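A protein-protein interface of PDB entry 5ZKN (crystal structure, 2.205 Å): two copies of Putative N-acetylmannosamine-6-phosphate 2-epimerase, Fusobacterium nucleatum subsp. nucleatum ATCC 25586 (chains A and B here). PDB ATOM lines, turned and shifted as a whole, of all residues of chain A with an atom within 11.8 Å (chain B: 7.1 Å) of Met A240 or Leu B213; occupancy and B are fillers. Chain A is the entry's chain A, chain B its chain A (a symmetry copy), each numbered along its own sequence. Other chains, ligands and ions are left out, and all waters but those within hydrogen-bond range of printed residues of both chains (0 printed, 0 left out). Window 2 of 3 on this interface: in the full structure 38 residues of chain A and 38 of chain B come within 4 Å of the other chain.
The backbone carbonyl oxygen of Glu A239 sits close to the side-chain amino group of Lys B210 (3.1 Å).
The backbone carbonyl oxygen (O) of Lys B28 is in hydrogen-bond range of the backbone NH (N) of Val B220 (3.2 Å).
N of Ile B30 lies within hydrogen-bond range of O of Val B220.
O of Ile B30 sits at hydrogen-bond distance from N of Val B222, 2.9 Å away.
The backbone carbonyl oxygen (O) of Leu B207 lies within hydrogen-bond range of the side-chain amino group (NZ) of Lys B211 (3.1 Å).
Among the printed residues, merely in contact across the chains: Lys A235 with Pro B206 (3.8 Å), Phe A236 with Leu B29 (3.7 Å), Phe A236 with Pro B206 (3.4 Å), Phe A236 with Ala B209 (3.9 Å), Phe A236 with Val B222 (3.7 Å), Val A237 with Leu B29 (3.9 Å), Glu A239 with Pro B206 (3.7 Å), Glu A239 with Leu B207 (3.6 Å), Met A240 with Lys B28 (3.6 Å), Met A240 with Leu B29 (3.8 Å), Met A240 with Leu B213 (3.6 Å) and Met A240 with Val B220 (3.6 Å).
Of the printed residues of chain B, Met A240 touches Lys B28, Leu B29, Leu B213 and Val B220.
Leu B213 touches just one residue of chain A: Met A240.
Lys B28 touches just one residue of chain A: Met A240.
Printed residues of chain A within 4 Å of Leu B29: Phe A236 (3.7 Å), Val A237 (3.9 Å) and Met A240 (3.8 Å).
Lys B210 touches just one residue of chain A: Glu A239 (3.0 Å).
No residue of chain A comes within 4 Å of Ala B212.
Of the printed residues of chain A, Val B222 touches Phe A236 (3.7 Å).
Of the printed residues of chain B, Lys A235 touches Pro B206.
Of the printed residues of chain B, Glu A239 touches Pro B206, Leu B207 and Lys B210.
Printed residues of chain B within 4 Å of Val A237: Leu B29.
Hydrophobic or aromatic side chains of chain B that line the printed part of chain A: Leu B29, Pro B206, Ala B209, Leu B213, Val B220 and Val B222.
Of the 12 printed residues of chain A, 5 touch a printed residue of chain B.
Among the printed residues, no Asp or Glu carboxylate lies within 4 Å of a Lys or Arg side-chain nitrogen of the other chain.
No position is printed for both chains.
Of the 13 pairs that touch across the chains among the printed residues, none has its exchanged pair printed and touching as well.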
ATOM      1  N   GLN A 230      16.247 -23.042   2.845  1.00  0.00           N
ATOM      2  CA  GLN A 230      17.692 -22.923   2.979  1.00  0.00           C
ATOM      3  C   GLN A 230      18.287 -22.269   1.741  1.00  0.00           C
ATOM      4  O   GLN A 230      19.290 -21.549   1.835  1.00  0.00           O
ATOM      5  CB  GLN A 230      18.338 -24.287   3.255  1.00  0.00           C
ATOM      6  CG  GLN A 230      18.706 -25.114   2.048  1.00  0.00           C
ATOM      7  CD  GLN A 230      19.810 -26.119   2.361  1.00  0.00           C
ATOM      8  OE1 GLN A 230      20.890 -25.751   2.839  1.00  0.00           O
ATOM      9  NE2 GLN A 230      19.540 -27.399   2.098  1.00  0.00           N
ATOM     10  N   GLN A 231      17.667 -22.467   0.579  1.00  0.00           N
ATOM     11  CA  GLN A 231      18.268 -21.864  -0.596  1.00  0.00           C
ATOM     12  C   GLN A 231      17.855 -20.400  -0.725  1.00  0.00           C
ATOM     13  O   GLN A 231      18.635 -19.583  -1.217  1.00  0.00           O
ATOM     14  CB  GLN A 231      17.964 -22.731  -1.831  1.00  0.00           C
ATOM     15  CG  GLN A 231      16.922 -22.299  -2.798  1.00  0.00           C
ATOM     16  CD  GLN A 231      16.834 -23.280  -3.961  1.00  0.00           C
ATOM     17  OE1 GLN A 231      17.285 -24.438  -3.858  1.00  0.00           O
ATOM     18  NE2 GLN A 231      16.279 -22.818  -5.084  1.00  0.00           N
ATOM     19  N   ILE A 232      16.686 -20.034  -0.201  1.00  0.00           N
ATOM     20  CA  ILE A 232      16.330 -18.624  -0.083  1.00  0.00           C
ATOM     21  C   ILE A 232      17.238 -17.938   0.938  1.00  0.00           C
ATOM     22  O   ILE A 232      17.714 -16.820   0.719  1.00  0.00           O
ATOM     23  CB  ILE A 232      14.844 -18.495   0.306  1.00  0.00           C
ATOM     24  CG1 ILE A 232      13.974 -19.348  -0.634  1.00  0.00           C
ATOM     25  CG2 ILE A 232      14.417 -17.020   0.307  1.00  0.00           C
ATOM     26  CD1 ILE A 232      12.561 -19.542  -0.145  1.00  0.00           C
ATOM     27  N   THR A 233      17.480 -18.597   2.072  1.00  0.00           N
ATOM     28  CA  THR A 233      18.362 -18.045   3.092  1.00  0.00           C
ATOM     29  C   THR A 233      19.758 -17.790   2.532  1.00  0.00           C
ATOM     30  O   THR A 233      20.351 -16.739   2.782  1.00  0.00           O
ATOM     31  CB  THR A 233      18.420 -19.006   4.284  1.00  0.00           C
ATOM     32  OG1 THR A 233      17.131 -19.059   4.900  1.00  0.00           O
ATOM     33  CG2 THR A 233      19.474 -18.576   5.309  1.00  0.00           C
ATOM     34  N   LYS A 234      20.284 -18.728   1.741  1.00  0.00           N
ATOM     35  CA  LYS A 234      21.632 -18.560   1.215  1.00  0.00           C
ATOM     36  C   LYS A 234      21.726 -17.356   0.274  1.00  0.00           C
ATOM     37  O   LYS A 234      22.795 -16.735   0.168  1.00  0.00           O
ATOM     38  CB  LYS A 234      22.077 -19.846   0.516  1.00  0.00           C
ATOM     39  CG  LYS A 234      23.516 -19.805  -0.023  1.00  0.00           C
ATOM     40  CD  LYS A 234      23.833 -21.084  -0.777  1.00  0.00           C
ATOM     41  CE  LYS A 234      25.302 -21.177  -1.148  1.00  0.00           C
ATOM     42  NZ  LYS A 234      25.678 -20.058  -2.023  1.00  0.00           N
ATOM     43  N   LYS A 235      20.626 -16.995  -0.402  1.00  0.00           N
ATOM     44  CA  LYS A 235      20.643 -15.785  -1.223  1.00  0.00           C
ATOM     45  C   LYS A 235      20.784 -14.535  -0.358  1.00  0.00           C
ATOM     46  O   LYS A 235      21.573 -13.639  -0.681  1.00  0.00           O
ATOM     47  CB  LYS A 235      19.395 -15.703  -2.109  1.00  0.00           C
ATOM     48  CG  LYS A 235      19.513 -16.502  -3.415  1.00  0.00           C
ATOM     49  CD  LYS A 235      18.516 -16.029  -4.461  1.00  0.00           C
ATOM     50  CE  LYS A 235      18.664 -16.768  -5.803  1.00  0.00           C
ATOM     51  NZ  LYS A 235      18.217 -18.199  -5.754  1.00  0.00           N
ATOM     52  N   PHE A 236      20.045 -14.466   0.753  1.00  0.00           N
ATOM     53  CA  PHE A 236      20.203 -13.355   1.688  1.00  0.00           C
ATOM     54  C   PHE A 236      21.625 -13.304   2.250  1.00  0.00           C
ATOM     55  O   PHE A 236      22.285 -12.255   2.211  1.00  0.00           O
ATOM     56  CB  PHE A 236      19.181 -13.479   2.822  1.00  0.00           C
ATOM     57  CG  PHE A 236      17.818 -12.969   2.464  1.00  0.00           C
ATOM     58  CD1 PHE A 236      16.895 -13.792   1.821  1.00  0.00           C
ATOM     59  CD2 PHE A 236      17.454 -11.669   2.768  1.00  0.00           C
ATOM     60  CE1 PHE A 236      15.628 -13.299   1.460  1.00  0.00           C
ATOM     61  CE2 PHE A 236      16.195 -11.183   2.433  1.00  0.00           C
ATOM     62  CZ  PHE A 236      15.282 -11.998   1.779  1.00  0.00           C
ATOM     63  N   VAL A 237      22.118 -14.442   2.753  1.00  0.00           N
ATOM     64  CA  VAL A 237      23.425 -14.485   3.410  1.00  0.00           C
ATOM     65  C   VAL A 237      24.521 -14.009   2.457  1.00  0.00           C
ATOM     66  O   VAL A 237      25.374 -13.187   2.819  1.00  0.00           O
ATOM     67  CB  VAL A 237      23.717 -15.902   3.945  1.00  0.00           C
ATOM     68  CG1 VAL A 237      25.186 -16.003   4.423  1.00  0.00           C
ATOM     69  CG2 VAL A 237      22.739 -16.263   5.081  1.00  0.00           C
ATOM     70  N   ASP A 238      24.502 -14.500   1.218  1.00  0.00           N
ATOM     71  CA  ASP A 238      25.595 -14.186   0.306  1.00  0.00           C
ATOM     72  C   ASP A 238      25.597 -12.728  -0.135  1.00  0.00           C
ATOM     73  O   ASP A 238      26.635 -12.248  -0.589  1.00  0.00           O
ATOM     74  CB  ASP A 238      25.540 -15.096  -0.920  1.00  0.00           C
ATOM     75  CG  ASP A 238      25.821 -16.543  -0.584  1.00  0.00           C
ATOM     76  OD1 ASP A 238      26.517 -16.807   0.423  1.00  0.00           O
ATOM     77  OD2 ASP A 238      25.334 -17.418  -1.333  1.00  0.00           O
ATOM     78  N   GLU A 239      24.479 -12.013  -0.028  1.00  0.00           N
ATOM     79  CA  GLU A 239      24.504 -10.589  -0.331  1.00  0.00           C
ATOM     80  C   GLU A 239      24.744  -9.737   0.903  1.00  0.00           C
ATOM     81  O   GLU A 239      24.825  -8.510   0.786  1.00  0.00           O
ATOM     82  CB  GLU A 239      23.213 -10.155  -1.030  1.00  0.00           C
ATOM     83  CG  GLU A 239      23.284 -10.285  -2.542  1.00  0.00           C
ATOM     84  CD  GLU A 239      22.625  -9.121  -3.232  1.00  0.00           C
ATOM     85  OE1 GLU A 239      22.131  -8.231  -2.509  1.00  0.00           O
ATOM     86  OE2 GLU A 239      22.605  -9.089  -4.485  1.00  0.00           O
ATOM     87  N   MET A 240      24.889 -10.355   2.071  1.00  0.00           N
ATOM     88  CA  MET A 240      25.231  -9.646   3.293  1.00  0.00           C
ATOM     89  C   MET A 240      26.725  -9.732   3.631  1.00  0.00           C
ATOM     90  O   MET A 240      27.128  -9.319   4.719  1.00  0.00           O
ATOM     91  CB  MET A 240      24.386 -10.175   4.457  1.00  0.00           C
ATOM     92  CG  MET A 240      22.895  -9.876   4.332  1.00  0.00           C
ATOM     93  SD  MET A 240      21.864 -10.754   5.560  1.00  0.00           S
ATOM     94  CE  MET A 240      22.115  -9.755   7.024  1.00  0.00           C
ATOM     95  N   LYS A 241      27.550 -10.251   2.731  1.00  0.00           N
ATOM     96  CA  LYS A 241      28.996 -10.252   2.940  1.00  0.00           C
ATOM     97  C   LYS A 241      29.680  -9.168   2.113  1.00  0.00           C
ATOM     98  O   LYS A 241      30.572  -8.471   2.601  1.00  0.00           O
ATOM     99  CB  LYS A 241      29.571 -11.624   2.604  1.00  0.00           C
ATOM    100  CG  LYS A 241      28.835 -12.757   3.307  1.00  0.00           C
ATOM    101  CD  LYS A 241      29.336 -14.113   2.853  1.00  0.00           C
ATOM    102  CE  LYS A 241      28.789 -15.233   3.730  1.00  0.00           C
ATOM    103  NZ  LYS A 241      29.216 -16.589   3.255  1.00  0.00           N
ATOM    104  N   ILE B  25      25.943 -12.777  16.461  1.00  0.00           N
ATOM    105  CA  ILE B  25      24.998 -12.311  15.437  1.00  0.00           C
ATOM    106  C   ILE B  25      25.463 -11.052  14.715  1.00  0.00           C
ATOM    107  O   ILE B  25      24.806 -10.645  13.733  1.00  0.00           O
ATOM    108  CB  ILE B  25      23.584 -12.079  16.012  1.00  0.00           C
ATOM    109  CG1 ILE B  25      23.633 -11.133  17.216  1.00  0.00           C
ATOM    110  CG2 ILE B  25      22.922 -13.386  16.365  1.00  0.00           C
ATOM    111  CD1 ILE B  25      22.263 -10.753  17.728  1.00  0.00           C
ATOM    112  N   ARG B  26      26.566 -10.436  15.155  1.00  0.00           N
ATOM    113  CA  ARG B  26      27.054  -9.185  14.582  1.00  0.00           C
ATOM    114  C   ARG B  26      27.225  -9.293  13.070  1.00  0.00           C
ATOM    115  O   ARG B  26      27.906 -10.194  12.575  1.00  0.00           O
ATOM    116  CB  ARG B  26      28.390  -8.800  15.230  1.00  0.00           C
ATOM    117  CG  ARG B  26      29.060  -7.628  14.537  1.00  0.00           C
ATOM    118  CD  ARG B  26      30.503  -7.393  15.007  1.00  0.00           C
ATOM    119  NE  ARG B  26      30.534  -6.782  16.334  1.00  0.00           N
ATOM    120  CZ  ARG B  26      30.431  -5.476  16.552  1.00  0.00           C
ATOM    121  NH1 ARG B  26      30.287  -4.649  15.519  1.00  0.00           N
ATOM    122  NH2 ARG B  26      30.469  -5.000  17.793  1.00  0.00           N
ATOM    123  N   GLY B  27      26.593  -8.368  12.337  1.00  0.00           N
ATOM    124  CA  GLY B  27      26.662  -8.375  10.887  1.00  0.00           C
ATOM    125  C   GLY B  27      26.059  -9.594  10.193  1.00  0.00           C
ATOM    126  O   GLY B  27      26.318  -9.817   9.005  1.00  0.00           O
ATOM    127  N   LYS B  28      25.248 -10.380  10.899  1.00  0.00           N
ATOM    128  CA  LYS B  28      24.725 -11.636  10.359  1.00  0.00           C
ATOM    129  C   LYS B  28      23.203 -11.596  10.182  1.00  0.00           C
ATOM    130  O   LYS B  28      22.516 -10.633  10.540  1.00  0.00           O
ATOM    131  CB  LYS B  28      25.118 -12.807  11.251  1.00  0.00           C
ATOM    132  CG  LYS B  28      26.608 -12.962  11.482  1.00  0.00           C
ATOM    133  CD  LYS B  28      27.320 -13.381  10.226  1.00  0.00           C
ATOM    134  CE  LYS B  28      28.651 -14.032  10.576  1.00  0.00           C
ATOM    135  NZ  LYS B  28      29.528 -14.229   9.380  1.00  0.00           N
ATOM    136  N   LEU B  29      22.682 -12.681   9.621  1.00  0.00           N
ATOM    137  CA  LEU B  29      21.255 -12.838   9.353  1.00  0.00           C
ATOM    138  C   LEU B  29      20.581 -13.637  10.463  1.00  0.00           C
ATOM    139  O   LEU B  29      21.034 -14.735  10.809  1.00  0.00           O
ATOM    140  CB  LEU B  29      21.029 -13.548   8.015  1.00  0.00           C
ATOM    141  CG  LEU B  29      19.560 -13.816   7.633  1.00  0.00           C
ATOM    142  CD1 LEU B  29      18.827 -12.491   7.505  1.00  0.00           C
ATOM    143  CD2 LEU B  29      19.468 -14.576   6.315  1.00  0.00           C
ATOM    144  N   ILE B  30      19.479 -13.108  10.987  1.00  0.00           N
ATOM    145  CA  ILE B  30      18.567 -13.852  11.850  1.00  0.00           C
ATOM    146  C   ILE B  30      17.289 -14.119  11.062  1.00  0.00           C
ATOM    147  O   ILE B  30      16.764 -13.216  10.404  1.00  0.00           O
ATOM    148  CB  ILE B  30      18.273 -13.076  13.142  1.00  0.00           C
ATOM    149  CG1 ILE B  30      19.590 -12.751  13.862  1.00  0.00           C
ATOM    150  CG2 ILE B  30      17.407 -13.892  14.067  1.00  0.00           C
ATOM    151  CD1 ILE B  30      19.431 -11.688  14.939  1.00  0.00           C
ATOM    152  N   LEU B 183      13.695   0.720   6.080  1.00  0.00           N
ATOM    153  CA  LEU B 183      15.022   1.288   5.912  1.00  0.00           C
ATOM    154  C   LEU B 183      15.046   2.775   6.241  1.00  0.00           C
ATOM    155  O   LEU B 183      16.028   3.269   6.807  1.00  0.00           O
ATOM    156  CB  LEU B 183      15.511   1.036   4.488  1.00  0.00           C
ATOM    157  CG  LEU B 183      15.570  -0.468   4.212  1.00  0.00           C
ATOM    158  CD1 LEU B 183      15.965  -0.722   2.768  1.00  0.00           C
ATOM    159  CD2 LEU B 183      16.539  -1.141   5.180  1.00  0.00           C
ATOM    160  N   LEU B 186      15.135   3.173   9.861  1.00  0.00           N
ATOM    161  CA  LEU B 186      16.356   2.554  10.377  1.00  0.00           C
ATOM    162  C   LEU B 186      17.509   3.554  10.422  1.00  0.00           C
ATOM    163  O   LEU B 186      18.187   3.693  11.449  1.00  0.00           O
ATOM    164  CB  LEU B 186      16.730   1.342   9.523  1.00  0.00           C
ATOM    165  CG  LEU B 186      18.072   0.663   9.859  1.00  0.00           C
ATOM    166  CD1 LEU B 186      18.010  -0.022  11.229  1.00  0.00           C
ATOM    167  CD2 LEU B 186      18.498  -0.354   8.785  1.00  0.00           C
ATOM    168  N   ALA B 199      17.767  -4.510  12.439  1.00  0.00           N
ATOM    169  CA  ALA B 199      16.795  -4.192  11.391  1.00  0.00           C
ATOM    170  C   ALA B 199      15.847  -5.370  11.234  1.00  0.00           C
ATOM    171  O   ALA B 199      16.286  -6.509  11.017  1.00  0.00           O
ATOM    172  CB  ALA B 199      17.486  -3.888  10.062  1.00  0.00           C
ATOM    173  N   PRO B 206      17.080  -9.803  -0.551  1.00  0.00           N
ATOM    174  CA  PRO B 206      18.508  -9.803  -0.186  1.00  0.00           C
ATOM    175  C   PRO B 206      19.146  -8.424  -0.287  1.00  0.00           C
ATOM    176  O   PRO B 206      20.023  -8.079   0.516  1.00  0.00           O
ATOM    177  CB  PRO B 206      19.121 -10.791  -1.188  1.00  0.00           C
ATOM    178  CG  PRO B 206      17.974 -11.738  -1.523  1.00  0.00           C
ATOM    179  CD  PRO B 206      16.740 -10.874  -1.515  1.00  0.00           C
ATOM    180  N   LEU B 207      18.686  -7.605  -1.233  1.00  0.00           N
ATOM    181  CA  LEU B 207      19.268  -6.289  -1.447  1.00  0.00           C
ATOM    182  C   LEU B 207      18.922  -5.349  -0.287  1.00  0.00           C
ATOM    183  O   LEU B 207      19.803  -4.662   0.246  1.00  0.00           O
ATOM    184  CB  LEU B 207      18.789  -5.779  -2.811  1.00  0.00           C
ATOM    185  CG  LEU B 207      19.673  -4.907  -3.663  1.00  0.00           C
ATOM    186  CD1 LEU B 207      19.093  -4.820  -5.165  1.00  0.00           C
ATOM    187  CD2 LEU B 207      20.189  -3.582  -3.031  1.00  0.00           C
ATOM    188  N   LYS B 208      17.661  -5.363   0.164  1.00  0.00           N
ATOM    189  CA  LYS B 208      17.273  -4.615   1.361  1.00  0.00           C
ATOM    190  C   LYS B 208      18.074  -5.039   2.583  1.00  0.00           C
ATOM    191  O   LYS B 208      18.345  -4.216   3.467  1.00  0.00           O
ATOM    192  CB  LYS B 208      15.786  -4.807   1.665  1.00  0.00           C
ATOM    193  CG  LYS B 208      14.818  -4.065   0.755  1.00  0.00           C
ATOM    194  CD  LYS B 208      13.403  -4.178   1.311  1.00  0.00           C
ATOM    195  CE  LYS B 208      12.382  -3.609   0.356  1.00  0.00           C
ATOM    196  NZ  LYS B 208      11.093  -3.470   1.057  1.00  0.00           N
ATOM    197  N   ALA B 209      18.431  -6.323   2.667  1.00  0.00           N
ATOM    198  CA  ALA B 209      19.224  -6.802   3.794  1.00  0.00           C
ATOM    199  C   ALA B 209      20.665  -6.304   3.702  1.00  0.00           C
ATOM    200  O   ALA B 209      21.288  -5.985   4.724  1.00  0.00           O
ATOM    201  CB  ALA B 209      19.156  -8.334   3.862  1.00  0.00           C
ATOM    202  N   LYS B 210      21.208  -6.209   2.489  1.00  0.00           N
ATOM    203  CA  LYS B 210      22.507  -5.560   2.333  1.00  0.00           C
ATOM    204  C   LYS B 210      22.426  -4.088   2.724  1.00  0.00           C
ATOM    205  O   LYS B 210      23.261  -3.592   3.491  1.00  0.00           O
ATOM    206  CB  LYS B 210      23.015  -5.708   0.899  1.00  0.00           C
ATOM    207  CG  LYS B 210      24.507  -5.515   0.759  1.00  0.00           C
ATOM    208  CD  LYS B 210      24.912  -5.330  -0.680  1.00  0.00           C
ATOM    209  CE  LYS B 210      26.429  -5.412  -0.845  1.00  0.00           C
ATOM    210  NZ  LYS B 210      26.878  -6.836  -0.918  1.00  0.00           N
ATOM    211  N   LYS B 211      21.409  -3.373   2.221  1.00  0.00           N
ATOM    212  CA  LYS B 211      21.299  -1.952   2.545  1.00  0.00           C
ATOM    213  C   LYS B 211      21.139  -1.729   4.038  1.00  0.00           C
ATOM    214  O   LYS B 211      21.606  -0.718   4.566  1.00  0.00           O
ATOM    215  CB  LYS B 211      20.139  -1.281   1.806  1.00  0.00           C
ATOM    216  CG  LYS B 211      20.462  -0.937   0.366  1.00  0.00           C
ATOM    217  CD  LYS B 211      19.380  -0.085  -0.280  1.00  0.00           C
ATOM    218  CE  LYS B 211      18.792  -0.830  -1.428  1.00  0.00           C
ATOM    219  NZ  LYS B 211      18.397  -2.175  -0.882  1.00  0.00           N
ATOM    220  N   ALA B 212      20.449  -2.639   4.726  1.00  0.00           N
ATOM    221  CA  ALA B 212      20.274  -2.484   6.163  1.00  0.00           C
ATOM    222  C   ALA B 212      21.621  -2.521   6.887  1.00  0.00           C
ATOM    223  O   ALA B 212      21.872  -1.705   7.786  1.00  0.00           O
ATOM    224  CB  ALA B 212      19.328  -3.565   6.691  1.00  0.00           C
ATOM    225  N   LEU B 213      22.507  -3.455   6.509  1.00  0.00           N
ATOM    226  CA  LEU B 213      23.848  -3.469   7.096  1.00  0.00           C
ATOM    227  C   LEU B 213      24.634  -2.231   6.686  1.00  0.00           C
ATOM    228  O   LEU B 213      25.342  -1.641   7.508  1.00  0.00           O
ATOM    229  CB  LEU B 213      24.613  -4.733   6.691  1.00  0.00           C
ATOM    230  CG  LEU B 213      24.181  -6.068   7.300  1.00  0.00           C
ATOM    231  CD1 LEU B 213      25.067  -7.200   6.785  1.00  0.00           C
ATOM    232  CD2 LEU B 213      24.188  -6.012   8.833  1.00  0.00           C
ATOM    233  N   GLU B 214      24.521  -1.823   5.415  1.00  0.00           N
ATOM    234  CA  GLU B 214      25.229  -0.632   4.946  1.00  0.00           C
ATOM    235  C   GLU B 214      24.741   0.622   5.660  1.00  0.00           C
ATOM    236  O   GLU B 214      25.523   1.549   5.891  1.00  0.00           O
ATOM    237  CB  GLU B 214      25.070  -0.482   3.430  1.00  0.00           C
ATOM    238  CG  GLU B 214      25.838  -1.527   2.619  1.00  0.00           C
ATOM    239  CD  GLU B 214      25.581  -1.438   1.116  1.00  0.00           C
ATOM    240  OE1 GLU B 214      26.231  -2.193   0.357  1.00  0.00           O
ATOM    241  OE2 GLU B 214      24.729  -0.623   0.693  1.00  0.00           O
ATOM    242  N   ILE B 215      23.462   0.662   6.034  1.00  0.00           N
ATOM    243  CA  ILE B 215      22.954   1.767   6.840  1.00  0.00           C
ATOM    244  C   ILE B 215      23.567   1.761   8.243  1.00  0.00           C
ATOM    245  O   ILE B 215      23.782   2.823   8.834  1.00  0.00           O
ATOM    246  CB  ILE B 215      21.413   1.710   6.877  1.00  0.00           C
ATOM    247  CG1 ILE B 215      20.834   2.123   5.529  1.00  0.00           C
ATOM    248  CG2 ILE B 215      20.854   2.603   7.969  1.00  0.00           C
ATOM    249  CD1 ILE B 215      19.333   1.958   5.458  1.00  0.00           C
ATOM    250  N   GLY B 216      23.869   0.589   8.800  1.00  0.00           N
ATOM    251  CA  GLY B 216      24.465   0.541  10.126  1.00  0.00           C
ATOM    252  C   GLY B 216      23.779  -0.388  11.109  1.00  0.00           C
ATOM    253  O   GLY B 216      24.060  -0.365  12.313  1.00  0.00           O
ATOM    254  N   ALA B 217      22.868  -1.216  10.613  1.00  0.00           N
ATOM    255  CA  ALA B 217      22.234  -2.195  11.481  1.00  0.00           C
ATOM    256  C   ALA B 217      23.286  -3.133  12.064  1.00  0.00           C
ATOM    257  O   ALA B 217      24.304  -3.437  11.431  1.00  0.00           O
ATOM    258  CB  ALA B 217      21.178  -2.989  10.711  1.00  0.00           C
ATOM    259  N   PHE B 218      23.042  -3.571  13.300  1.00  0.00           N
ATOM    260  CA  PHE B 218      23.923  -4.527  13.954  1.00  0.00           C
ATOM    261  C   PHE B 218      23.684  -5.951  13.437  1.00  0.00           C
ATOM    262  O   PHE B 218      24.626  -6.760  13.381  1.00  0.00           O
ATOM    263  CB  PHE B 218      23.721  -4.427  15.474  1.00  0.00           C
ATOM    264  CG  PHE B 218      24.631  -5.308  16.279  1.00  0.00           C
ATOM    265  CD1 PHE B 218      24.262  -6.605  16.594  1.00  0.00           C
ATOM    266  CD2 PHE B 218      25.859  -4.833  16.727  1.00  0.00           C
ATOM    267  CE1 PHE B 218      25.108  -7.430  17.340  1.00  0.00           C
ATOM    268  CE2 PHE B 218      26.714  -5.650  17.469  1.00  0.00           C
ATOM    269  CZ  PHE B 218      26.337  -6.954  17.779  1.00  0.00           C
ATOM    270  N   ALA B 219      22.439  -6.268  13.061  1.00  0.00           N
ATOM    271  CA  ALA B 219      22.073  -7.537  12.440  1.00  0.00           C
ATOM    272  C   ALA B 219      20.744  -7.315  11.743  1.00  0.00           C
ATOM    273  O   ALA B 219      20.098  -6.278  11.921  1.00  0.00           O
ATOM    274  CB  ALA B 219      21.988  -8.682  13.461  1.00  0.00           C
ATOM    275  N   VAL B 220      20.339  -8.292  10.934  1.00  0.00           N
ATOM    276  CA  VAL B 220      19.122  -8.171  10.131  1.00  0.00           C
ATOM    277  C   VAL B 220      18.259  -9.402  10.391  1.00  0.00           C
ATOM    278  O   VAL B 220      18.769 -10.530  10.420  1.00  0.00           O
ATOM    279  CB  VAL B 220      19.438  -8.015   8.626  1.00  0.00           C
ATOM    280  CG1 VAL B 220      18.150  -7.903   7.798  1.00  0.00           C
ATOM    281  CG2 VAL B 220      20.316  -6.797   8.380  1.00  0.00           C
ATOM    282  N   VAL B 221      16.964  -9.180  10.608  1.00  0.00           N
ATOM    283  CA  VAL B 221      15.967 -10.243  10.763  1.00  0.00           C
ATOM    284  C   VAL B 221      15.118 -10.287   9.495  1.00  0.00           C
ATOM    285  O   VAL B 221      14.598  -9.258   9.058  1.00  0.00           O
ATOM    286  CB  VAL B 221      15.081 -10.022  12.007  1.00  0.00           C
ATOM    287  CG1 VAL B 221      13.866 -10.934  11.982  1.00  0.00           C
ATOM    288  CG2 VAL B 221      15.892 -10.211  13.331  1.00  0.00           C
ATOM    289  N   VAL B 222      14.994 -11.478   8.903  1.00  0.00           N
ATOM    290  CA  VAL B 222      14.130 -11.742   7.753  1.00  0.00           C
ATOM    291  C   VAL B 222      13.127 -12.820   8.151  1.00  0.00           C
ATOM    292  O   VAL B 222      13.503 -13.858   8.717  1.00  0.00           O
ATOM    293  CB  VAL B 222      14.943 -12.184   6.522  1.00  0.00           C
ATOM    294  CG1 VAL B 222      14.013 -12.536   5.360  1.00  0.00           C
ATOM    295  CG2 VAL B 222      15.951 -11.088   6.128  1.00  0.00           C
